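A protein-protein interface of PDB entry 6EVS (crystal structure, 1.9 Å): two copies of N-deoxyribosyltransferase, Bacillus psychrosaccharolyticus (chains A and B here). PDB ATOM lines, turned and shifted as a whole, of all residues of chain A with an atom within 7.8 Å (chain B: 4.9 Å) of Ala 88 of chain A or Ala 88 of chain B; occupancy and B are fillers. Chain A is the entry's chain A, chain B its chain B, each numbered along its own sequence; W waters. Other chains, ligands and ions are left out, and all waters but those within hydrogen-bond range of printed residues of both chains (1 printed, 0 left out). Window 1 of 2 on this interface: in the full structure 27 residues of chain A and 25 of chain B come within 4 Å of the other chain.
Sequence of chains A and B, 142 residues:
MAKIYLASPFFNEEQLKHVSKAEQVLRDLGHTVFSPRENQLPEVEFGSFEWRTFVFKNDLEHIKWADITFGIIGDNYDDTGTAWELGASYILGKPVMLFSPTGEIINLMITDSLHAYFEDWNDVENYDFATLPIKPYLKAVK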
ATOM      1  N   LEU A  60      19.582  -1.245  26.846  1.00  0.00           N
ATOM      2  CA  LEU A  60      18.494  -0.294  26.634  1.00  0.00           C
ATOM      3  C   LEU A  60      18.574   0.878  27.613  1.00  0.00           C
ATOM      4  O   LEU A  60      18.429   2.041  27.216  1.00  0.00           O
ATOM      5  CB  LEU A  60      17.148  -1.013  26.757  1.00  0.00           C
ATOM      6  CG  LEU A  60      15.893  -0.253  26.332  1.00  0.00           C
ATOM      7  CD1 LEU A  60      16.046   0.294  24.906  1.00  0.00           C
ATOM      8  CD2 LEU A  60      14.668  -1.151  26.446  1.00  0.00           C
ATOM      9  N   ILE A  63      21.082   3.214  26.297  1.00  0.00           N
ATOM     10  CA  ILE A  63      20.591   4.040  25.197  1.00  0.00           C
ATOM     11  C   ILE A  63      19.797   5.208  25.753  1.00  0.00           C
ATOM     12  O   ILE A  63      19.922   6.348  25.284  1.00  0.00           O
ATOM     13  CB  ILE A  63      19.732   3.216  24.218  1.00  0.00           C
ATOM     14  CG1 ILE A  63      20.497   2.023  23.652  1.00  0.00           C
ATOM     15  CG2 ILE A  63      19.220   4.110  23.088  1.00  0.00           C
ATOM     16  CD1 ILE A  63      19.629   1.238  22.681  1.00  0.00           C
ATOM     17  N   LYS A  64      18.975   4.941  26.772  1.00  0.00           N
ATOM     18  CA  LYS A  64      18.182   5.998  27.403  1.00  0.00           C
ATOM     19  C   LYS A  64      19.064   7.011  28.126  1.00  0.00           C
ATOM     20  O   LYS A  64      18.766   8.218  28.124  1.00  0.00           O
ATOM     21  CB  LYS A  64      17.174   5.370  28.360  1.00  0.00           C
ATOM     22  CG  LYS A  64      16.022   4.697  27.646  1.00  0.00           C
ATOM     23  CD  LYS A  64      15.372   3.629  28.506  1.00  0.00           C
ATOM     24  CE  LYS A  64      14.199   3.008  27.764  1.00  0.00           C
ATOM     25  NZ  LYS A  64      13.361   2.127  28.621  1.00  0.00           N
ATOM     26  N   THR A  69      23.325   8.354  20.069  1.00  0.00           N
ATOM     27  CA  THR A  69      23.664   6.996  19.682  1.00  0.00           C
ATOM     28  C   THR A  69      24.537   7.031  18.434  1.00  0.00           C
ATOM     29  O   THR A  69      24.119   7.536  17.382  1.00  0.00           O
ATOM     30  CB  THR A  69      22.439   6.137  19.421  1.00  0.00           C
ATOM     31  OG1 THR A  69      21.727   5.950  20.652  1.00  0.00           O
ATOM     32  CG2 THR A  69      22.852   4.736  18.759  1.00  0.00           C
ATOM     33  N   GLY A  81      20.986  -6.434  15.512  1.00  0.00           N
ATOM     34  CA  GLY A  81      20.816  -5.761  16.792  1.00  0.00           C
ATOM     35  C   GLY A  81      21.169  -4.290  16.708  1.00  0.00           C
ATOM     36  O   GLY A  81      20.502  -3.449  17.315  1.00  0.00           O
ATOM     37  N   THR A  82      22.221  -3.954  15.947  1.00  0.00           N
ATOM     38  CA  THR A  82      22.567  -2.541  15.773  1.00  0.00           C
ATOM     39  C   THR A  82      21.420  -1.785  15.119  1.00  0.00           C
ATOM     40  O   THR A  82      21.009  -0.718  15.599  1.00  0.00           O
ATOM     41  CB  THR A  82      23.846  -2.400  14.940  1.00  0.00           C
ATOM     42  OG1 THR A  82      24.948  -2.944  15.678  1.00  0.00           O
ATOM     43  CG2 THR A  82      24.126  -0.917  14.630  1.00  0.00           C
ATOM     44  N   ALA A  83      20.862  -2.345  14.043  1.00  0.00           N
ATOM     45  CA  ALA A  83      19.737  -1.693  13.372  1.00  0.00           C
ATOM     46  C   ALA A  83      18.556  -1.501  14.326  1.00  0.00           C
ATOM     47  O   ALA A  83      17.917  -0.439  14.335  1.00  0.00           O
ATOM     48  CB  ALA A  83      19.317  -2.518  12.150  1.00  0.00           C
ATOM     49  N   TRP A  84      18.275  -2.518  15.152  1.00  0.00           N
ATOM     50  CA  TRP A  84      17.240  -2.412  16.188  1.00  0.00           C
ATOM     51  C   TRP A  84      17.539  -1.260  17.142  1.00  0.00           C
ATOM     52  O   TRP A  84      16.649  -0.456  17.482  1.00  0.00           O
ATOM     53  CB  TRP A  84      17.151  -3.764  16.933  1.00  0.00           C
ATOM     54  CG  TRP A  84      16.003  -3.908  17.919  1.00  0.00           C
ATOM     55  CD1 TRP A  84      14.821  -4.571  17.715  1.00  0.00           C
ATOM     56  CD2 TRP A  84      15.939  -3.376  19.250  1.00  0.00           C
ATOM     57  NE1 TRP A  84      14.015  -4.462  18.833  1.00  0.00           N
ATOM     58  CE2 TRP A  84      14.682  -3.750  19.794  1.00  0.00           C
ATOM     59  CE3 TRP A  84      16.823  -2.635  20.044  1.00  0.00           C
ATOM     60  CZ2 TRP A  84      14.287  -3.406  21.102  1.00  0.00           C
ATOM     61  CZ3 TRP A  84      16.411  -2.271  21.353  1.00  0.00           C
ATOM     62  CH2 TRP A  84      15.156  -2.659  21.853  1.00  0.00           C
ATOM     63  N   GLU A  85      18.793  -1.142  17.572  1.00  0.00           N
ATOM     64  CA  GLU A  85      19.146  -0.075  18.506  1.00  0.00           C
ATOM     65  C   GLU A  85      19.043   1.303  17.868  1.00  0.00           C
ATOM     66  O   GLU A  85      18.759   2.275  18.573  1.00  0.00           O
ATOM     67  CB  GLU A  85      20.556  -0.301  19.054  1.00  0.00           C
ATOM     68  CG  GLU A  85      20.631  -1.591  19.873  1.00  0.00           C
ATOM     69  CD  GLU A  85      22.043  -1.963  20.271  1.00  0.00           C
ATOM     70  OE1 GLU A  85      23.015  -1.587  19.573  1.00  0.00           O
ATOM     71  OE2 GLU A  85      22.170  -2.659  21.293  1.00  0.00           O
ATOM     72  N   LEU A  86      19.292   1.429  16.563  1.00  0.00           N
ATOM     73  CA  LEU A  86      19.097   2.746  15.938  1.00  0.00           C
ATOM     74  C   LEU A  86      17.617   3.088  15.807  1.00  0.00           C
ATOM     75  O   LEU A  86      17.235   4.249  15.969  1.00  0.00           O
ATOM     76  CB  LEU A  86      19.780   2.807  14.561  1.00  0.00           C
ATOM     77  CG  LEU A  86      21.286   2.554  14.564  1.00  0.00           C
ATOM     78  CD1 LEU A  86      21.765   2.316  13.127  1.00  0.00           C
ATOM     79  CD2 LEU A  86      22.029   3.732  15.191  1.00  0.00           C
ATOM     80  N   GLY A  87      16.764   2.101  15.517  1.00  0.00           N
ATOM     81  CA  GLY A  87      15.331   2.374  15.494  1.00  0.00           C
ATOM     82  C   GLY A  87      14.794   2.774  16.864  1.00  0.00           C
ATOM     83  O   GLY A  87      14.049   3.748  17.001  1.00  0.00           O
ATOM     84  N   ALA A  88      15.174   2.028  17.909  1.00  0.00           N
ATOM     85  CA  ALA A  88      14.806   2.442  19.260  1.00  0.00           C
ATOM     86  C   ALA A  88      15.318   3.846  19.567  1.00  0.00           C
ATOM     87  O   ALA A  88      14.573   4.695  20.082  1.00  0.00           O
ATOM     88  CB  ALA A  88      15.343   1.434  20.281  1.00  0.00           C
ATOM     89  N   SER A  89      16.592   4.107  19.259  1.00  0.00           N
ATOM     90  CA  SER A  89      17.186   5.419  19.526  1.00  0.00           C
ATOM     91  C   SER A  89      16.375   6.535  18.896  1.00  0.00           C
ATOM     92  O   SER A  89      16.136   7.573  19.525  1.00  0.00           O
ATOM     93  CB  SER A  89      18.634   5.471  19.008  1.00  0.00           C
ATOM     94  OG  SER A  89      19.451   4.592  19.785  1.00  0.00           O
ATOM     95  N   TYR A  90      15.994   6.357  17.631  1.00  0.00           N
ATOM     96  CA  TYR A  90      15.242   7.377  16.910  1.00  0.00           C
ATOM     97  C   TYR A  90      13.935   7.700  17.618  1.00  0.00           C
ATOM     98  O   TYR A  90      13.616   8.873  17.847  1.00  0.00           O
ATOM     99  CB  TYR A  90      14.972   6.902  15.481  1.00  0.00           C
ATOM    100  CG  TYR A  90      14.229   7.926  14.653  1.00  0.00           C
ATOM    101  CD1 TYR A  90      14.862   9.085  14.218  1.00  0.00           C
ATOM    102  CD2 TYR A  90      12.894   7.738  14.309  1.00  0.00           C
ATOM    103  CE1 TYR A  90      14.194  10.026  13.441  1.00  0.00           C
ATOM    104  CE2 TYR A  90      12.215   8.681  13.547  1.00  0.00           C
ATOM    105  CZ  TYR A  90      12.871   9.808  13.112  1.00  0.00           C
ATOM    106  OH  TYR A  90      12.187  10.738  12.368  1.00  0.00           O
ATOM    107  N   ILE A  91      13.161   6.672  17.984  1.00  0.00           N
ATOM    108  CA  ILE A  91      11.921   6.942  18.719  1.00  0.00           C
ATOM    109  C   ILE A  91      12.220   7.574  20.073  1.00  0.00           C
ATOM    110  O   ILE A  91      11.467   8.438  20.539  1.00  0.00           O
ATOM    111  CB  ILE A  91      11.063   5.673  18.871  1.00  0.00           C
ATOM    112  CG1 ILE A  91      10.780   5.034  17.498  1.00  0.00           C
ATOM    113  CG2 ILE A  91       9.732   6.016  19.632  1.00  0.00           C
ATOM    114  CD1 ILE A  91      10.148   6.009  16.482  1.00  0.00           C
ATOM    115  N   LEU A  92      13.313   7.178  20.726  1.00  0.00           N
ATOM    116  CA  LEU A  92      13.645   7.776  22.019  1.00  0.00           C
ATOM    117  C   LEU A  92      14.144   9.210  21.884  1.00  0.00           C
ATOM    118  O   LEU A  92      14.434   9.851  22.900  1.00  0.00           O
ATOM    119  CB  LEU A  92      14.700   6.933  22.735  1.00  0.00           C
ATOM    120  CG  LEU A  92      14.274   5.571  23.321  1.00  0.00           C
ATOM    121  CD1 LEU A  92      15.504   4.750  23.681  1.00  0.00           C
ATOM    122  CD2 LEU A  92      13.377   5.816  24.556  1.00  0.00           C
ATOM    123  N   GLY A  93      14.250   9.725  20.664  1.00  0.00           N
ATOM    124  CA  GLY A  93      14.661  11.110  20.468  1.00  0.00           C
ATOM    125  C   GLY A  93      16.143  11.341  20.635  1.00  0.00           C
ATOM    126  O   GLY A  93      16.565  12.480  20.849  1.00  0.00           O
ATOM    127  N   LYS A  94      16.962  10.274  20.544  1.00  0.00           N
ATOM    128  CA  LYS A  94      18.410  10.431  20.587  1.00  0.00           C
ATOM    129  C   LYS A  94      18.923  10.735  19.185  1.00  0.00           C
ATOM    130  O   LYS A  94      18.635   9.965  18.258  1.00  0.00           O
ATOM    131  CB  LYS A  94      19.082   9.157  21.093  1.00  0.00           C
ATOM    132  CG  LYS A  94      18.410   8.615  22.319  1.00  0.00           C
ATOM    133  CD  LYS A  94      18.633   9.559  23.435  1.00  0.00           C
ATOM    134  CE  LYS A  94      18.215   8.910  24.785  1.00  0.00           C
ATOM    135  NZ  LYS A  94      18.292   9.989  25.810  1.00  0.00           N
ATOM    136  N   VAL A  96      20.994  10.362  16.064  1.00  0.00           N
ATOM    137  CA  VAL A  96      21.750   9.208  15.592  1.00  0.00           C
ATOM    138  C   VAL A  96      22.882   9.683  14.697  1.00  0.00           C
ATOM    139  O   VAL A  96      22.647  10.381  13.707  1.00  0.00           O
ATOM    140  CB  VAL A  96      20.853   8.205  14.847  1.00  0.00           C
ATOM    141  CG1 VAL A  96      21.717   7.191  14.111  1.00  0.00           C
ATOM    142  CG2 VAL A  96      19.921   7.514  15.808  1.00  0.00           C
ATOM    143  N   MET A 109      15.296   3.231   5.848  1.00  0.00           N
ATOM    144  CA  MET A 109      14.807   3.503   7.203  1.00  0.00           C
ATOM    145  C   MET A 109      15.931   4.044   8.078  1.00  0.00           C
ATOM    146  O   MET A 109      15.699   4.921   8.916  1.00  0.00           O
ATOM    147  CB  MET A 109      14.170   2.255   7.830  1.00  0.00           C
ATOM    148  CG  MET A 109      13.010   1.671   7.002  1.00  0.00           C
ATOM    149  SD  MET A 109      11.691   2.871   6.638  1.00  0.00           S
ATOM    150  CE  MET A 109      11.064   3.159   8.307  1.00  0.00           C
ATOM    151  N   TRP B  84      15.252  -2.307  12.275  1.00  0.00           N
ATOM    152  CA  TRP B  84      14.969  -0.920  12.649  1.00  0.00           C
ATOM    153  C   TRP B  84      13.502  -0.729  13.028  1.00  0.00           C
ATOM    154  O   TRP B  84      13.183  -0.103  14.051  1.00  0.00           O
ATOM    155  CB  TRP B  84      15.354   0.003  11.472  1.00  0.00           C
ATOM    156  CG  TRP B  84      15.355   1.498  11.825  1.00  0.00           C
ATOM    157  CD1 TRP B  84      16.444   2.268  12.141  1.00  0.00           C
ATOM    158  CD2 TRP B  84      14.226   2.374  11.857  1.00  0.00           C
ATOM    159  NE1 TRP B  84      16.055   3.564  12.391  1.00  0.00           N
ATOM    160  CE2 TRP B  84      14.698   3.657  12.225  1.00  0.00           C
ATOM    161  CE3 TRP B  84      12.861   2.200  11.623  1.00  0.00           C
ATOM    162  CZ2 TRP B  84      13.853   4.757  12.369  1.00  0.00           C
ATOM    163  CZ3 TRP B  84      12.013   3.303  11.783  1.00  0.00           C
ATOM    164  CH2 TRP B  84      12.518   4.562  12.139  1.00  0.00           C
ATOM    165  N   GLU B  85      12.587  -1.225  12.186  1.00  0.00           N
ATOM    166  CA  GLU B  85      11.171  -1.039  12.468  1.00  0.00           C
ATOM    167  C   GLU B  85      10.733  -1.806  13.704  1.00  0.00           C
ATOM    168  O   GLU B  85       9.820  -1.347  14.402  1.00  0.00           O
ATOM    169  CB  GLU B  85      10.300  -1.413  11.261  1.00  0.00           C
ATOM    170  CG  GLU B  85      10.794  -0.835   9.938  1.00  0.00           C
ATOM    171  CD  GLU B  85       9.957  -1.277   8.744  1.00  0.00           C
ATOM    172  OE1 GLU B  85       9.530  -0.417   7.960  1.00  0.00           O
ATOM    173  OE2 GLU B  85       9.682  -2.478   8.609  1.00  0.00           O
ATOM    174  N   LEU B  86      11.368  -2.959  14.007  1.00  0.00           N
ATOM    175  CA  LEU B  86      11.014  -3.662  15.247  1.00  0.00           C
ATOM    176  C   LEU B  86      11.470  -2.878  16.475  1.00  0.00           C
ATOM    177  O   LEU B  86      10.749  -2.807  17.484  1.00  0.00           O
ATOM    178  CB  LEU B  86      11.633  -5.076  15.262  1.00  0.00           C
ATOM    179  CG  LEU B  86      11.246  -6.045  14.142  1.00  0.00           C
ATOM    180  CD1 LEU B  86      11.891  -7.425  14.374  1.00  0.00           C
ATOM    181  CD2 LEU B  86       9.737  -6.187  14.062  1.00  0.00           C
ATOM    182  N   GLY B  87      12.690  -2.339  16.432  1.00  0.00           N
ATOM    183  CA  GLY B  87      13.155  -1.481  17.513  1.00  0.00           C
ATOM    184  C   GLY B  87      12.284  -0.247  17.702  1.00  0.00           C
ATOM    185  O   GLY B  87      11.892   0.091  18.824  1.00  0.00           O
ATOM    186  N   ALA B  88      11.972   0.453  16.608  1.00  0.00           N
ATOM    187  CA  ALA B  88      11.035   1.572  16.719  1.00  0.00           C
ATOM    188  C   ALA B  88       9.702   1.127  17.319  1.00  0.00           C
ATOM    189  O   ALA B  88       9.142   1.810  18.185  1.00  0.00           O
ATOM    190  CB  ALA B  88      10.805   2.201  15.336  1.00  0.00           C
ATOM    191  N   SER B  89       9.170  -0.009  16.866  1.00  0.00           N
ATOM    192  CA  SER B  89       7.855  -0.439  17.333  1.00  0.00           C
ATOM    193  C   SER B  89       7.880  -0.718  18.828  1.00  0.00           C
ATOM    194  O   SER B  89       6.937  -0.377  19.543  1.00  0.00           O
ATOM    195  CB  SER B  89       7.391  -1.685  16.577  1.00  0.00           C
ATOM    196  OG  SER B  89       7.320  -1.419  15.195  1.00  0.00           O
ATOM    197  N   TYR B  90       8.969  -1.316  19.312  1.00  0.00           N
ATOM    198  CA  TYR B  90       9.099  -1.596  20.738  1.00  0.00           C
ATOM    199  C   TYR B  90       9.018  -0.320  21.562  1.00  0.00           C
ATOM    200  O   TYR B  90       8.262  -0.252  22.538  1.00  0.00           O
ATOM    201  CB  TYR B  90      10.414  -2.329  21.008  1.00  0.00           C
ATOM    202  CG  TYR B  90      10.606  -2.662  22.476  1.00  0.00           C
ATOM    203  CD1 TYR B  90       9.771  -3.569  23.104  1.00  0.00           C
ATOM    204  CD2 TYR B  90      11.629  -2.084  23.223  1.00  0.00           C
ATOM    205  CE1 TYR B  90       9.951  -3.914  24.444  1.00  0.00           C
ATOM    206  CE2 TYR B  90      11.811  -2.422  24.575  1.00  0.00           C
ATOM    207  CZ  TYR B  90      10.968  -3.327  25.164  1.00  0.00           C
ATOM    208  OH  TYR B  90      11.126  -3.656  26.502  1.00  0.00           O
ATOM    209  N   ILE B  91       9.773   0.717  21.178  1.00  0.00           N
ATOM    210  CA  ILE B  91       9.727   1.967  21.954  1.00  0.00           C
ATOM    211  C   ILE B  91       8.387   2.657  21.805  1.00  0.00           C
ATOM    212  O   ILE B  91       7.892   3.284  22.760  1.00  0.00           O
ATOM    213  CB  ILE B  91      10.878   2.905  21.557  1.00  0.00           C
ATOM    214  CG1 ILE B  91      12.210   2.187  21.715  1.00  0.00           C
ATOM    215  CG2 ILE B  91      10.857   4.163  22.438  1.00  0.00           C
ATOM    216  CD1 ILE B  91      12.467   1.705  23.201  1.00  0.00           C
ATOM    217  N   LEU B  92       7.760   2.554  20.630  1.00  0.00           N
ATOM    218  CA  LEU B  92       6.431   3.135  20.463  1.00  0.00           C
ATOM    219  C   LEU B  92       5.370   2.406  21.274  1.00  0.00           C
ATOM    220  O   LEU B  92       4.231   2.869  21.331  1.00  0.00           O
ATOM    221  CB  LEU B  92       6.018   3.127  18.984  1.00  0.00           C
ATOM    222  CG  LEU B  92       6.770   4.087  18.064  1.00  0.00           C
ATOM    223  CD1 LEU B  92       6.508   3.707  16.623  1.00  0.00           C
ATOM    224  CD2 LEU B  92       6.281   5.524  18.342  1.00  0.00           C
HETATM  225  O   HOH W   1      17.900   5.529  13.256  1.00  0.00           O
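Along chain A the printed residues that touch a printed residue of chain B span positions 60 to 109. Of the 9 printed residues of chain B, 8 touch a printed residue of chain A. Hydrophobic or aromatic side chains of chain B within 4 Å of the printed part of chain A: Trp 84, Ala 88, Tyr 90, Ile 91 and Leu 92. Among the printed residues, 18 pairs touch across the chains.
Water W1 bridges the indole nitrogen (NE1) of Trp 84 of chain B (2.8 Å) and the backbone carbonyl oxygen (O) of Leu 86 of chain A (3.1 Å).
NE1 of Trp 84 of chain B touches C of Leu 86 of chain A, 3.8 Å away. Trp 84 of chain B touches Gly 87 of chain A. Gly 87 of chain A touches Ala 88 of chain B (C to N, 3.7 Å). N of Ala 88 of chain A touches C of Gly 87 of chain B, 3.7 Å away. Trp 84 of chain B touches Tyr 90 of chain A. Ala 88 of chain B touches Ile 91 of chain A. Ile 91 of chain A touches Ile 91 of chain B. CG2 of Ile 91 of chain A touches CD2 of Leu 92 of chain B, at 3.7 Å. Ile 91 of chain B touches Leu 92 of chain A. Met 109 of chain A touches Trp 84 of chain B.
Of the printed residues of chain B, Ala 83 of chain A touches Trp 84. Of chain B, only Gly 87, Ala 88 and Ile 91 come within 4 Å of Ala 88 of chain A. Ser 89 of chain A touches none of the printed residues of chain B. Of the printed residues of chain B, Leu 92 of chain A touches Ile 91. Val 96 of chain A touches none of the printed residues of chain B. Printed residues of chain A within 4 Å of Leu 86 of chain B: Trp 84.
Trp 84 of chain A touches Leu 86 of chain B, and with the chains exchanged Leu 86 of chain A touches Trp 84 of chain B. Trp 84 of chain A touches Gly 87 of chain B, and with the chains exchanged Gly 87 of chain A touches Trp 84 of chain B. Gly 87 of chain A touches Ala 88 of chain B, and with the chains exchanged Ala 88 of chain A touches Gly 87 of chain B. Ala 88 of chain B touches its own counterpart, Ala 88 of chain A. Of the 18 pairs that touch across the chains among the printed residues, 14 have their exchanged pair printed and touching as well.
The backbone carbonyl oxygen (O) of Glu 85 of chain B lies within hydrogen-bond range of the side-chain hydroxyl (OG) of Ser 89 of chain B, at 2.6 Å.
The indole nitrogen (NE1) of Trp 84 of chain A sits close to the backbone NH (N) of Gly 87 of chain B.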
